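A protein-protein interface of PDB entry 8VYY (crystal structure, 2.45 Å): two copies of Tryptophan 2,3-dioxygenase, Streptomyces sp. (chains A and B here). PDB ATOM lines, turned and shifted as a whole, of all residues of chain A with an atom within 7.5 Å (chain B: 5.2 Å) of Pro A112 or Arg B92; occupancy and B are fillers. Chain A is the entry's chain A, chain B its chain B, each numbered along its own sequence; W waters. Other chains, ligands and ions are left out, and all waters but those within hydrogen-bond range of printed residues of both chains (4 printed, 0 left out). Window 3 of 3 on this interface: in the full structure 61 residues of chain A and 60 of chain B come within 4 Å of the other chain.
The backbone carbonyl oxygen (O) of His A110 lies within hydrogen-bond range of the guanidinium group (NH2) of Arg B92 (3.0 Å).
The guanidinium group (NH1) of Arg B73 is in salt-bridge range of the side-chain carboxylate (OD1) of Asp A49 (2.9 Å).
The guanidinium group (NH1) of Arg B92 lies within salt-bridge range of the side-chain carboxylate (OD1) of Asp A49.
The guanidinium group of Arg B73 is in hydrogen-bond range of the backbone carbonyl oxygen of Pro A48 (3.5 Å).
OD2 of Asp A49 sits at hydrogen-bond distance from OG of Ser A115 (2.8 Å).
The backbone NH (N) of Asp A49 sits at hydrogen-bond distance from a ring nitrogen (ND1) of His A47, 2.9 Å away.
NH1 of Arg B73 lies within salt-bridge range of OE1 of Glu B70.
NH1 of Arg B92 is in salt-bridge range of OE2 of Glu B70, at 3.1 Å.
SD of Met B89 sits close to NE of Arg B73, 3.7 Å away.
Among the printed residues, pairs that only touch across the chains: His A110 with Asp B91 (3.4 Å), Phe A52 with Arg B92 (3.6 Å), Leu A106 with Gly B95 (3.7 Å), Phe A52 with Glu B70 (3.7 Å), Pro A112 with Arg B92 (3.8 Å) and Leu A106 with Leu B96 (3.8 Å).
Of the printed residues of chain B, Phe A52 touches Glu B70 and Arg B92.
Of chain B, only Arg B92 (3.8 Å) comes within 4 Å of Pro A112.
Of the printed residues of chain A, Arg B73 touches Pro A48 and Asp A49.
Of the printed residues of chain A, Asp B91 touches His A110.
Arg B92 touches four residues of chain A.
Printed residues of chain A within 4 Å of Gly B95: Leu A106.
The nearest printed residue of chain B that does not touch Pro A112 is Arg B88 (5.7 Å).
Of the 13 printed residues of chain B, 6 touch a printed residue of chain A.
Printed residues of chain B that touch a printed residue of chain A: Glu B70, Arg B73, Asp B91, Arg B92, Gly B95 and Leu B96.
Hydrophobic or aromatic side chains of chain B that line the printed part of chain A: Leu B96.
Printed residues of chain A that touch a printed residue of chain B: Pro A48, Asp A49, Phe A52, Leu A106, His A110 and Pro A112.
Hydrophobic or aromatic side chains of chain A within 4 Å of the printed part of chain B: Pro A48, Phe A52, Leu A106, His A110 and Pro A112.
Among the printed residues, Asp or Glu carboxylates within 4 Å of a Lys or Arg side-chain nitrogen of the other chain: Asp A49 with Arg B73 (2.9 Å) and Asp A49 with Arg B92 (2.8 Å).
No position is printed for both chains.
Water W1 lies within hydrogen-bond range of the backbone carbonyl oxygen (O) of His A110 and the guanidinium group (NH2) of Arg B92.
Water W3 lies within hydrogen-bond range of the side-chain carboxylate of Asp A49 (2.6 Å) and the guanidinium group of Arg B73 (3.1 Å).
Water W2 lies within hydrogen-bond range of O of Pro A48, OE2 of Glu B70 and N of Phe A52.
Water W4 lies within hydrogen-bond range of the guanidinium group (NE) of Arg B92, the backbone carbonyl oxygen (O) of Arg B88 and the backbone carbonyl oxygen (O) of His A110.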
ATOM      1  N   HIS A  47     -23.394  21.950  36.248  1.00  0.00           N
ATOM      2  CA  HIS A  47     -22.598  21.943  35.033  1.00  0.00           C
ATOM      3  C   HIS A  47     -23.307  22.809  34.006  1.00  0.00           C
ATOM      4  O   HIS A  47     -24.541  22.852  33.991  1.00  0.00           O
ATOM      5  CB  HIS A  47     -22.427  20.504  34.516  1.00  0.00           C
ATOM      6  CG  HIS A  47     -21.398  20.356  33.439  1.00  0.00           C
ATOM      7  ND1 HIS A  47     -21.570  20.867  32.170  1.00  0.00           N
ATOM      8  CD2 HIS A  47     -20.192  19.737  33.436  1.00  0.00           C
ATOM      9  CE1 HIS A  47     -20.508  20.586  31.435  1.00  0.00           C
ATOM     10  NE2 HIS A  47     -19.659  19.893  32.178  1.00  0.00           N
ATOM     11  N   PRO A  48     -22.568  23.520  33.151  1.00  0.00           N
ATOM     12  CA  PRO A  48     -23.238  24.350  32.132  1.00  0.00           C
ATOM     13  C   PRO A  48     -24.054  23.552  31.119  1.00  0.00           C
ATOM     14  O   PRO A  48     -24.981  24.119  30.530  1.00  0.00           O
ATOM     15  CB  PRO A  48     -22.077  25.102  31.457  1.00  0.00           C
ATOM     16  CG  PRO A  48     -20.837  24.317  31.814  1.00  0.00           C
ATOM     17  CD  PRO A  48     -21.108  23.737  33.171  1.00  0.00           C
ATOM     18  N   ASP A  49     -23.769  22.262  30.914  1.00  0.00           N
ATOM     19  CA  ASP A  49     -24.526  21.438  29.981  1.00  0.00           C
ATOM     20  C   ASP A  49     -25.760  20.799  30.615  1.00  0.00           C
ATOM     21  O   ASP A  49     -26.415  19.974  29.973  1.00  0.00           O
ATOM     22  CB  ASP A  49     -23.622  20.362  29.373  1.00  0.00           C
ATOM     23  CG  ASP A  49     -22.605  20.943  28.396  1.00  0.00           C
ATOM     24  OD1 ASP A  49     -22.951  21.920  27.710  1.00  0.00           O
ATOM     25  OD2 ASP A  49     -21.452  20.453  28.325  1.00  0.00           O
ATOM     26  N   GLN A  50     -26.114  21.189  31.838  1.00  0.00           N
ATOM     27  CA  GLN A  50     -27.227  20.555  32.540  1.00  0.00           C
ATOM     28  C   GLN A  50     -28.581  20.993  31.990  1.00  0.00           C
ATOM     29  O   GLN A  50     -29.489  20.166  31.847  1.00  0.00           O
ATOM     30  CB  GLN A  50     -27.137  20.880  34.030  1.00  0.00           C
ATOM     31  CG  GLN A  50     -27.951  19.969  34.937  1.00  0.00           C
ATOM     32  CD  GLN A  50     -27.998  20.484  36.369  1.00  0.00           C
ATOM     33  OE1 GLN A  50     -26.972  20.889  36.929  1.00  0.00           O
ATOM     34  NE2 GLN A  50     -29.186  20.465  36.970  1.00  0.00           N
ATOM     35  N   ARG A  51     -28.742  22.298  31.739  1.00  0.00           N
ATOM     36  CA  ARG A  51     -29.946  22.833  31.111  1.00  0.00           C
ATOM     37  C   ARG A  51     -30.268  22.110  29.800  1.00  0.00           C
ATOM     38  O   ARG A  51     -31.403  21.669  29.573  1.00  0.00           O
ATOM     39  CB  ARG A  51     -29.742  24.330  30.860  1.00  0.00           C
ATOM     40  CG  ARG A  51     -30.109  25.212  32.032  1.00  0.00           C
ATOM     41  CD  ARG A  51     -31.601  25.114  32.293  1.00  0.00           C
ATOM     42  NE  ARG A  51     -32.080  26.222  33.106  1.00  0.00           N
ATOM     43  CZ  ARG A  51     -32.185  27.477  32.686  1.00  0.00           C
ATOM     44  NH1 ARG A  51     -31.888  27.817  31.440  1.00  0.00           N
ATOM     45  NH2 ARG A  51     -32.605  28.411  33.538  1.00  0.00           N
ATOM     46  N   PHE A  52     -29.264  21.978  28.930  1.00  0.00           N
ATOM     47  CA  PHE A  52     -29.434  21.285  27.658  1.00  0.00           C
ATOM     48  C   PHE A  52     -29.935  19.873  27.884  1.00  0.00           C
ATOM     49  O   PHE A  52     -30.890  19.418  27.231  1.00  0.00           O
ATOM     50  CB  PHE A  52     -28.100  21.274  26.909  1.00  0.00           C
ATOM     51  CG  PHE A  52     -28.152  20.628  25.548  1.00  0.00           C
ATOM     52  CD1 PHE A  52     -29.091  21.023  24.606  1.00  0.00           C
ATOM     53  CD2 PHE A  52     -27.231  19.655  25.193  1.00  0.00           C
ATOM     54  CE1 PHE A  52     -29.126  20.448  23.347  1.00  0.00           C
ATOM     55  CE2 PHE A  52     -27.263  19.078  23.932  1.00  0.00           C
ATOM     56  CZ  PHE A  52     -28.212  19.484  23.006  1.00  0.00           C
ATOM     57  N   PHE A  53     -29.298  19.170  28.823  1.00  0.00           N
ATOM     58  CA  PHE A  53     -29.702  17.817  29.171  1.00  0.00           C
ATOM     59  C   PHE A  53     -31.168  17.782  29.580  1.00  0.00           C
ATOM     60  O   PHE A  53     -31.945  16.972  29.065  1.00  0.00           O
ATOM     61  CB  PHE A  53     -28.774  17.307  30.283  1.00  0.00           C
ATOM     62  CG  PHE A  53     -29.063  15.917  30.760  1.00  0.00           C
ATOM     63  CD1 PHE A  53     -28.424  14.827  30.185  1.00  0.00           C
ATOM     64  CD2 PHE A  53     -29.932  15.698  31.836  1.00  0.00           C
ATOM     65  CE1 PHE A  53     -28.669  13.533  30.643  1.00  0.00           C
ATOM     66  CE2 PHE A  53     -30.185  14.403  32.304  1.00  0.00           C
ATOM     67  CZ  PHE A  53     -29.549  13.322  31.698  1.00  0.00           C
ATOM     68  N   LEU A 106     -30.167  15.357  19.180  1.00  0.00           N
ATOM     69  CA  LEU A 106     -29.522  16.566  19.679  1.00  0.00           C
ATOM     70  C   LEU A 106     -28.443  16.221  20.689  1.00  0.00           C
ATOM     71  O   LEU A 106     -27.339  16.775  20.640  1.00  0.00           O
ATOM     72  CB  LEU A 106     -30.563  17.492  20.305  1.00  0.00           C
ATOM     73  CG  LEU A 106     -31.126  18.586  19.397  1.00  0.00           C
ATOM     74  CD1 LEU A 106     -32.084  19.406  20.184  1.00  0.00           C
ATOM     75  CD2 LEU A 106     -30.005  19.468  18.902  1.00  0.00           C
ATOM     76  N   LEU A 107     -28.735  15.293  21.605  1.00  0.00           N
ATOM     77  CA  LEU A 107     -27.728  14.868  22.569  1.00  0.00           C
ATOM     78  C   LEU A 107     -26.582  14.129  21.887  1.00  0.00           C
ATOM     79  O   LEU A 107     -25.413  14.330  22.237  1.00  0.00           O
ATOM     80  CB  LEU A 107     -28.373  13.989  23.635  1.00  0.00           C
ATOM     81  CG  LEU A 107     -29.320  14.713  24.588  1.00  0.00           C
ATOM     82  CD1 LEU A 107     -29.558  13.849  25.776  1.00  0.00           C
ATOM     83  CD2 LEU A 107     -28.712  16.034  25.025  1.00  0.00           C
ATOM     84  N   THR A 108     -26.890  13.258  20.922  1.00  0.00           N
ATOM     85  CA  THR A 108     -25.827  12.549  20.218  1.00  0.00           C
ATOM     86  C   THR A 108     -24.854  13.519  19.558  1.00  0.00           C
ATOM     87  O   THR A 108     -23.644  13.279  19.542  1.00  0.00           O
ATOM     88  CB  THR A 108     -26.417  11.634  19.154  1.00  0.00           C
ATOM     89  OG1 THR A 108     -27.414  10.806  19.739  1.00  0.00           O
ATOM     90  CG2 THR A 108     -25.340  10.773  18.550  1.00  0.00           C
ATOM     91  N   ASP A 109     -25.364  14.618  19.006  1.00  0.00           N
ATOM     92  CA  ASP A 109     -24.541  15.512  18.201  1.00  0.00           C
ATOM     93  C   ASP A 109     -23.860  16.600  19.013  1.00  0.00           C
ATOM     94  O   ASP A 109     -22.807  17.085  18.598  1.00  0.00           O
ATOM     95  CB  ASP A 109     -25.387  16.155  17.090  1.00  0.00           C
ATOM     96  CG  ASP A 109     -25.761  15.160  16.009  1.00  0.00           C
ATOM     97  OD1 ASP A 109     -25.079  14.121  15.921  1.00  0.00           O
ATOM     98  OD2 ASP A 109     -26.739  15.386  15.260  1.00  0.00           O
ATOM     99  N   HIS A 110     -24.417  16.989  20.162  1.00  0.00           N
ATOM    100  CA  HIS A 110     -23.916  18.150  20.877  1.00  0.00           C
ATOM    101  C   HIS A 110     -23.597  17.916  22.344  1.00  0.00           C
ATOM    102  O   HIS A 110     -22.964  18.781  22.952  1.00  0.00           O
ATOM    103  CB  HIS A 110     -24.917  19.317  20.762  1.00  0.00           C
ATOM    104  CG  HIS A 110     -25.287  19.632  19.349  1.00  0.00           C
ATOM    105  ND1 HIS A 110     -24.400  20.198  18.458  1.00  0.00           N
ATOM    106  CD2 HIS A 110     -26.434  19.421  18.656  1.00  0.00           C
ATOM    107  CE1 HIS A 110     -24.985  20.327  17.279  1.00  0.00           C
ATOM    108  NE2 HIS A 110     -26.222  19.868  17.372  1.00  0.00           N
ATOM    109  N   LEU A 111     -24.007  16.807  22.935  1.00  0.00           N
ATOM    110  CA  LEU A 111     -23.664  16.599  24.338  1.00  0.00           C
ATOM    111  C   LEU A 111     -22.284  15.968  24.427  1.00  0.00           C
ATOM    112  O   LEU A 111     -22.105  14.824  23.984  1.00  0.00           O
ATOM    113  CB  LEU A 111     -24.688  15.716  25.044  1.00  0.00           C
ATOM    114  CG  LEU A 111     -24.420  15.452  26.528  1.00  0.00           C
ATOM    115  CD1 LEU A 111     -24.692  16.689  27.367  1.00  0.00           C
ATOM    116  CD2 LEU A 111     -25.232  14.262  27.038  1.00  0.00           C
ATOM    117  N   PRO A 112     -21.297  16.672  24.993  1.00  0.00           N
ATOM    118  CA  PRO A 112     -19.951  16.087  25.151  1.00  0.00           C
ATOM    119  C   PRO A 112     -19.965  14.912  26.121  1.00  0.00           C
ATOM    120  O   PRO A 112     -20.527  14.997  27.219  1.00  0.00           O
ATOM    121  CB  PRO A 112     -19.114  17.251  25.697  1.00  0.00           C
ATOM    122  CG  PRO A 112     -19.944  18.508  25.418  1.00  0.00           C
ATOM    123  CD  PRO A 112     -21.367  18.049  25.514  1.00  0.00           C
ATOM    124  N   GLN A 113     -19.346  13.804  25.702  1.00  0.00           N
ATOM    125  CA  GLN A 113     -19.251  12.649  26.585  1.00  0.00           C
ATOM    126  C   GLN A 113     -18.631  13.024  27.927  1.00  0.00           C
ATOM    127  O   GLN A 113     -19.092  12.579  28.985  1.00  0.00           O
ATOM    128  CB  GLN A 113     -18.440  11.540  25.926  1.00  0.00           C
ATOM    129  CG  GLN A 113     -18.047  10.496  26.920  1.00  0.00           C
ATOM    130  CD  GLN A 113     -17.348   9.334  26.295  1.00  0.00           C
ATOM    131  OE1 GLN A 113     -16.473   9.511  25.438  1.00  0.00           O
ATOM    132  NE2 GLN A 113     -17.714   8.122  26.725  1.00  0.00           N
ATOM    133  N   HIS A 114     -17.613  13.882  27.904  1.00  0.00           N
ATOM    134  CA  HIS A 114     -16.955  14.268  29.147  1.00  0.00           C
ATOM    135  C   HIS A 114     -17.879  15.052  30.078  1.00  0.00           C
ATOM    136  O   HIS A 114     -17.757  14.930  31.301  1.00  0.00           O
ATOM    137  CB  HIS A 114     -15.681  15.059  28.834  1.00  0.00           C
ATOM    138  CG  HIS A 114     -14.778  15.231  30.014  1.00  0.00           C
ATOM    139  ND1 HIS A 114     -15.059  16.106  31.042  1.00  0.00           N
ATOM    140  CD2 HIS A 114     -13.600  14.639  30.329  1.00  0.00           C
ATOM    141  CE1 HIS A 114     -14.096  16.043  31.943  1.00  0.00           C
ATOM    142  NE2 HIS A 114     -13.196  15.165  31.533  1.00  0.00           N
ATOM    143  N   SER A 115     -18.808  15.858  29.545  1.00  0.00           N
ATOM    144  CA  SER A 115     -19.764  16.515  30.439  1.00  0.00           C
ATOM    145  C   SER A 115     -20.795  15.530  30.950  1.00  0.00           C
ATOM    146  O   SER A 115     -21.283  15.672  32.077  1.00  0.00           O
ATOM    147  CB  SER A 115     -20.499  17.669  29.750  1.00  0.00           C
ATOM    148  OG  SER A 115     -19.656  18.391  28.894  1.00  0.00           O
ATOM    149  N   LEU A 116     -21.167  14.554  30.126  1.00  0.00           N
ATOM    150  CA  LEU A 116     -22.148  13.580  30.577  1.00  0.00           C
ATOM    151  C   LEU A 116     -21.581  12.744  31.717  1.00  0.00           C
ATOM    152  O   LEU A 116     -22.274  12.491  32.709  1.00  0.00           O
ATOM    153  CB  LEU A 116     -22.602  12.715  29.399  1.00  0.00           C
ATOM    154  CG  LEU A 116     -23.651  11.616  29.582  1.00  0.00           C
ATOM    155  CD1 LEU A 116     -23.001  10.272  29.961  1.00  0.00           C
ATOM    156  CD2 LEU A 116     -24.732  12.041  30.598  1.00  0.00           C
ATOM    157  N   LEU A 117     -20.300  12.363  31.627  1.00  0.00           N
ATOM    158  CA  LEU A 117     -19.699  11.555  32.690  1.00  0.00           C
ATOM    159  C   LEU A 117     -19.570  12.348  33.990  1.00  0.00           C
ATOM    160  O   LEU A 117     -19.888  11.828  35.066  1.00  0.00           O
ATOM    161  CB  LEU A 117     -18.350  11.001  32.235  1.00  0.00           C
ATOM    162  CG  LEU A 117     -18.381  10.094  30.995  1.00  0.00           C
ATOM    163  CD1 LEU A 117     -17.000   9.570  30.654  1.00  0.00           C
ATOM    164  CD2 LEU A 117     -19.356   8.942  31.145  1.00  0.00           C
ATOM    165  N   MET A 118     -19.148  13.620  33.913  1.00  0.00           N
ATOM    166  CA  MET A 118     -19.113  14.454  35.112  1.00  0.00           C
ATOM    167  C   MET A 118     -20.509  14.690  35.661  1.00  0.00           C
ATOM    168  O   MET A 118     -20.701  14.760  36.880  1.00  0.00           O
ATOM    169  CB  MET A 118     -18.446  15.807  34.838  1.00  0.00           C
ATOM    170  CG  MET A 118     -17.095  15.717  34.170  1.00  0.00           C
ATOM    171  SD  MET A 118     -15.816  15.035  35.261  1.00  0.00           S
ATOM    172  CE  MET A 118     -15.738  13.318  34.704  1.00  0.00           C
ATOM    173  N   MET A 119     -21.493  14.844  34.780  1.00  0.00           N
ATOM    174  CA  MET A 119     -22.849  15.088  35.251  1.00  0.00           C
ATOM    175  C   MET A 119     -23.437  13.822  35.861  1.00  0.00           C
ATOM    176  O   MET A 119     -24.124  13.881  36.889  1.00  0.00           O
ATOM    177  CB  MET A 119     -23.712  15.594  34.092  1.00  0.00           C
ATOM    178  CG  MET A 119     -23.809  17.105  34.014  1.00  0.00           C
ATOM    179  SD  MET A 119     -24.820  17.698  32.631  1.00  0.00           S
ATOM    180  CE  MET A 119     -24.439  16.522  31.352  1.00  0.00           C
ATOM    181  N   SER A 209     -22.256   6.183  22.289  1.00  0.00           N
ATOM    182  CA  SER A 209     -21.268   7.248  22.188  1.00  0.00           C
ATOM    183  C   SER A 209     -20.976   7.906  23.531  1.00  0.00           C
ATOM    184  O   SER A 209     -20.046   8.711  23.616  1.00  0.00           O
ATOM    185  CB  SER A 209     -21.738   8.306  21.177  1.00  0.00           C
ATOM    186  OG  SER A 209     -22.742   9.157  21.730  1.00  0.00           O
ATOM    187  N   GLN A 210     -21.752   7.601  24.570  1.00  0.00           N
ATOM    188  CA  GLN A 210     -21.588   8.218  25.881  1.00  0.00           C
ATOM    189  C   GLN A 210     -21.112   7.248  26.945  1.00  0.00           C
ATOM    190  O   GLN A 210     -20.225   7.581  27.727  1.00  0.00           O
ATOM    191  CB  GLN A 210     -22.903   8.856  26.327  1.00  0.00           C
ATOM    192  CG  GLN A 210     -23.475   9.830  25.316  1.00  0.00           C
ATOM    193  CD  GLN A 210     -22.827  11.196  25.400  1.00  0.00           C
ATOM    194  OE1 GLN A 210     -22.264  11.549  26.428  1.00  0.00           O
ATOM    195  NE2 GLN A 210     -22.920  11.981  24.326  1.00  0.00           N
ATOM    196  N   GLU B  70     -27.587  29.082  25.409  1.00  0.00           N
ATOM    197  CA  GLU B  70     -26.361  28.741  24.686  1.00  0.00           C
ATOM    198  C   GLU B  70     -25.740  29.961  24.007  1.00  0.00           C
ATOM    199  O   GLU B  70     -24.515  30.017  23.834  1.00  0.00           O
ATOM    200  CB  GLU B  70     -26.644  27.625  23.665  1.00  0.00           C
ATOM    201  CG  GLU B  70     -27.319  26.368  24.257  1.00  0.00           C
ATOM    202  CD  GLU B  70     -26.455  25.623  25.312  1.00  0.00           C
ATOM    203  OE1 GLU B  70     -25.306  26.049  25.584  1.00  0.00           O
ATOM    204  OE2 GLU B  70     -26.920  24.601  25.872  1.00  0.00           O
ATOM    205  N   ARG B  73     -23.601  31.708  26.510  1.00  0.00           N
ATOM    206  CA  ARG B  73     -22.308  31.034  26.574  1.00  0.00           C
ATOM    207  C   ARG B  73     -21.419  31.404  25.394  1.00  0.00           C
ATOM    208  O   ARG B  73     -20.208  31.603  25.562  1.00  0.00           O
ATOM    209  CB  ARG B  73     -22.499  29.522  26.645  1.00  0.00           C
ATOM    210  CG  ARG B  73     -23.181  29.085  27.937  1.00  0.00           C
ATOM    211  CD  ARG B  73     -23.399  27.572  27.987  1.00  0.00           C
ATOM    212  NE  ARG B  73     -22.154  26.812  27.924  1.00  0.00           N
ATOM    213  CZ  ARG B  73     -22.101  25.493  27.769  1.00  0.00           C
ATOM    214  NH1 ARG B  73     -23.200  24.770  27.640  1.00  0.00           N
ATOM    215  NH2 ARG B  73     -20.916  24.886  27.729  1.00  0.00           N
ATOM    216  N   VAL B  87     -18.020  27.889  18.581  1.00  0.00           N
ATOM    217  CA  VAL B  87     -18.571  27.120  17.467  1.00  0.00           C
ATOM    218  C   VAL B  87     -19.607  26.130  17.968  1.00  0.00           C
ATOM    219  O   VAL B  87     -20.721  26.046  17.438  1.00  0.00           O
ATOM    220  CB  VAL B  87     -17.448  26.396  16.696  1.00  0.00           C
ATOM    221  CG1 VAL B  87     -18.021  25.599  15.553  1.00  0.00           C
ATOM    222  CG2 VAL B  87     -16.470  27.394  16.146  1.00  0.00           C
ATOM    223  N   ARG B  88     -19.254  25.374  19.007  1.00  0.00           N
ATOM    224  CA  ARG B  88     -20.141  24.320  19.477  1.00  0.00           C
ATOM    225  C   ARG B  88     -21.437  24.900  20.004  1.00  0.00           C
ATOM    226  O   ARG B  88     -22.509  24.306  19.825  1.00  0.00           O
ATOM    227  CB  ARG B  88     -19.451  23.496  20.554  1.00  0.00           C
ATOM    228  CG  ARG B  88     -18.293  22.684  20.040  1.00  0.00           C
ATOM    229  CD  ARG B  88     -17.878  21.698  21.109  1.00  0.00           C
ATOM    230  NE  ARG B  88     -16.600  21.092  20.783  1.00  0.00           N
ATOM    231  CZ  ARG B  88     -15.434  21.588  21.163  1.00  0.00           C
ATOM    232  NH1 ARG B  88     -15.365  22.692  21.890  1.00  0.00           N
ATOM    233  NH2 ARG B  88     -14.313  20.958  20.809  1.00  0.00           N
ATOM    234  N   MET B  89     -21.359  26.068  20.641  1.00  0.00           N
ATOM    235  CA  MET B  89     -22.558  26.719  21.155  1.00  0.00           C
ATOM    236  C   MET B  89     -23.500  27.114  20.026  1.00  0.00           C
ATOM    237  O   MET B  89     -24.726  26.955  20.142  1.00  0.00           O
ATOM    238  CB  MET B  89     -22.159  27.940  21.989  1.00  0.00           C
ATOM    239  CG  MET B  89     -21.326  27.569  23.205  1.00  0.00           C
ATOM    240  SD  MET B  89     -22.210  26.377  24.232  1.00  0.00           S
ATOM    241  CE  MET B  89     -21.179  24.927  23.994  1.00  0.00           C
ATOM    242  N   PHE B  90     -22.944  27.621  18.915  1.00  0.00           N
ATOM    243  CA  PHE B  90     -23.789  28.028  17.801  1.00  0.00           C
ATOM    244  C   PHE B  90     -24.389  26.818  17.104  1.00  0.00           C
ATOM    245  O   PHE B  90     -25.556  26.851  16.703  1.00  0.00           O
ATOM    246  CB  PHE B  90     -23.003  28.892  16.809  1.00  0.00           C
ATOM    247  CG  PHE B  90     -22.754  30.290  17.304  1.00  0.00           C
ATOM    248  CD1 PHE B  90     -23.820  31.140  17.587  1.00  0.00           C
ATOM    249  CD2 PHE B  90     -21.452  30.752  17.505  1.00  0.00           C
ATOM    250  CE1 PHE B  90     -23.595  32.439  18.054  1.00  0.00           C
ATOM    251  CE2 PHE B  90     -21.223  32.047  17.978  1.00  0.00           C
ATOM    252  CZ  PHE B  90     -22.298  32.891  18.253  1.00  0.00           C
ATOM    253  N   ASP B  91     -23.606  25.739  16.968  1.00  0.00           N
ATOM    254  CA  ASP B  91     -24.106  24.503  16.364  1.00  0.00           C
ATOM    255  C   ASP B  91     -25.254  23.920  17.181  1.00  0.00           C
ATOM    256  O   ASP B  91     -26.258  23.457  16.621  1.00  0.00           O
ATOM    257  CB  ASP B  91     -22.971  23.493  16.268  1.00  0.00           C
ATOM    258  CG  ASP B  91     -22.054  23.738  15.068  1.00  0.00           C
ATOM    259  OD1 ASP B  91     -22.363  24.619  14.229  1.00  0.00           O
ATOM    260  OD2 ASP B  91     -20.978  23.086  15.005  1.00  0.00           O
ATOM    261  N   ARG B  92     -25.117  23.929  18.511  1.00  0.00           N
ATOM    262  CA  ARG B  92     -26.172  23.431  19.386  1.00  0.00           C
ATOM    263  C   ARG B  92     -27.425  24.293  19.269  1.00  0.00           C
ATOM    264  O   ARG B  92     -28.544  23.772  19.188  1.00  0.00           O
ATOM    265  CB  ARG B  92     -25.662  23.394  20.829  1.00  0.00           C
ATOM    266  CG  ARG B  92     -26.640  22.805  21.832  1.00  0.00           C
ATOM    267  CD  ARG B  92     -26.092  22.890  23.260  1.00  0.00           C
ATOM    268  NE  ARG B  92     -24.816  22.191  23.413  1.00  0.00           N
ATOM    269  CZ  ARG B  92     -24.252  21.943  24.587  1.00  0.00           C
ATOM    270  NH1 ARG B  92     -24.836  22.308  25.714  1.00  0.00           N
ATOM    271  NH2 ARG B  92     -23.078  21.308  24.634  1.00  0.00           N
ATOM    272  N   ALA B  93     -27.249  25.619  19.237  1.00  0.00           N
ATOM    273  CA  ALA B  93     -28.380  26.524  19.076  1.00  0.00           C
ATOM    274  C   ALA B  93     -29.122  26.258  17.766  1.00  0.00           C
ATOM    275  O   ALA B  93     -30.357  26.304  17.723  1.00  0.00           O
ATOM    276  CB  ALA B  93     -27.883  27.968  19.130  1.00  0.00           C
ATOM    277  N   THR B  94     -28.385  25.984  16.688  1.00  0.00           N
ATOM    278  CA  THR B  94     -29.023  25.664  15.419  1.00  0.00           C
ATOM    279  C   THR B  94     -29.854  24.400  15.539  1.00  0.00           C
ATOM    280  O   THR B  94     -30.993  24.354  15.067  1.00  0.00           O
ATOM    281  CB  THR B  94     -27.970  25.507  14.319  1.00  0.00           C
ATOM    282  OG1 THR B  94     -27.319  26.758  14.125  1.00  0.00           O
ATOM    283  CG2 THR B  94     -28.614  25.121  13.002  1.00  0.00           C
ATOM    284  N   GLY B  95     -29.295  23.356  16.164  1.00  0.00           N
ATOM    285  CA  GLY B  95     -30.052  22.127  16.343  1.00  0.00           C
ATOM    286  C   GLY B  95     -31.345  22.368  17.094  1.00  0.00           C
ATOM    287  O   GLY B  95     -32.384  21.796  16.762  1.00  0.00           O
ATOM    288  N   LEU B  96     -31.305  23.242  18.101  1.00  0.00           N
ATOM    289  CA  LEU B  96     -32.512  23.532  18.868  1.00  0.00           C
ATOM    290  C   LEU B  96     -33.514  24.323  18.042  1.00  0.00           C
ATOM    291  O   LEU B  96     -34.724  24.096  18.140  1.00  0.00           O
ATOM    292  CB  LEU B  96     -32.156  24.306  20.129  1.00  0.00           C
ATOM    293  CG  LEU B  96     -31.417  23.526  21.210  1.00  0.00           C
ATOM    294  CD1 LEU B  96     -30.556  24.506  22.031  1.00  0.00           C
ATOM    295  CD2 LEU B  96     -32.430  22.732  22.074  1.00  0.00           C
ATOM    296  N   SER B  97     -33.025  25.271  17.240  1.00  0.00           N
ATOM    297  CA  SER B  97     -33.884  26.029  16.342  1.00  0.00           C
ATOM    298  C   SER B  97     -34.624  25.115  15.364  1.00  0.00           C
ATOM    299  O   SER B  97     -35.813  25.327  15.068  1.00  0.00           O
ATOM    300  CB  SER B  97     -33.035  27.051  15.588  1.00  0.00           C
ATOM    301  OG  SER B  97     -33.826  27.813  14.692  1.00  0.00           O
HETATM  302  O   HOH W   1     -20.990  20.330  22.372  1.00  0.00           O
HETATM  303  O   HOH W   2     -26.908  23.725  28.669  1.00  0.00           O
HETATM  304  O   HOH W   3     -19.655  22.048  27.350  1.00  0.00           O
HETATM  305  O   HOH W   4     -22.622  21.919  21.540  1.00  0.00           O
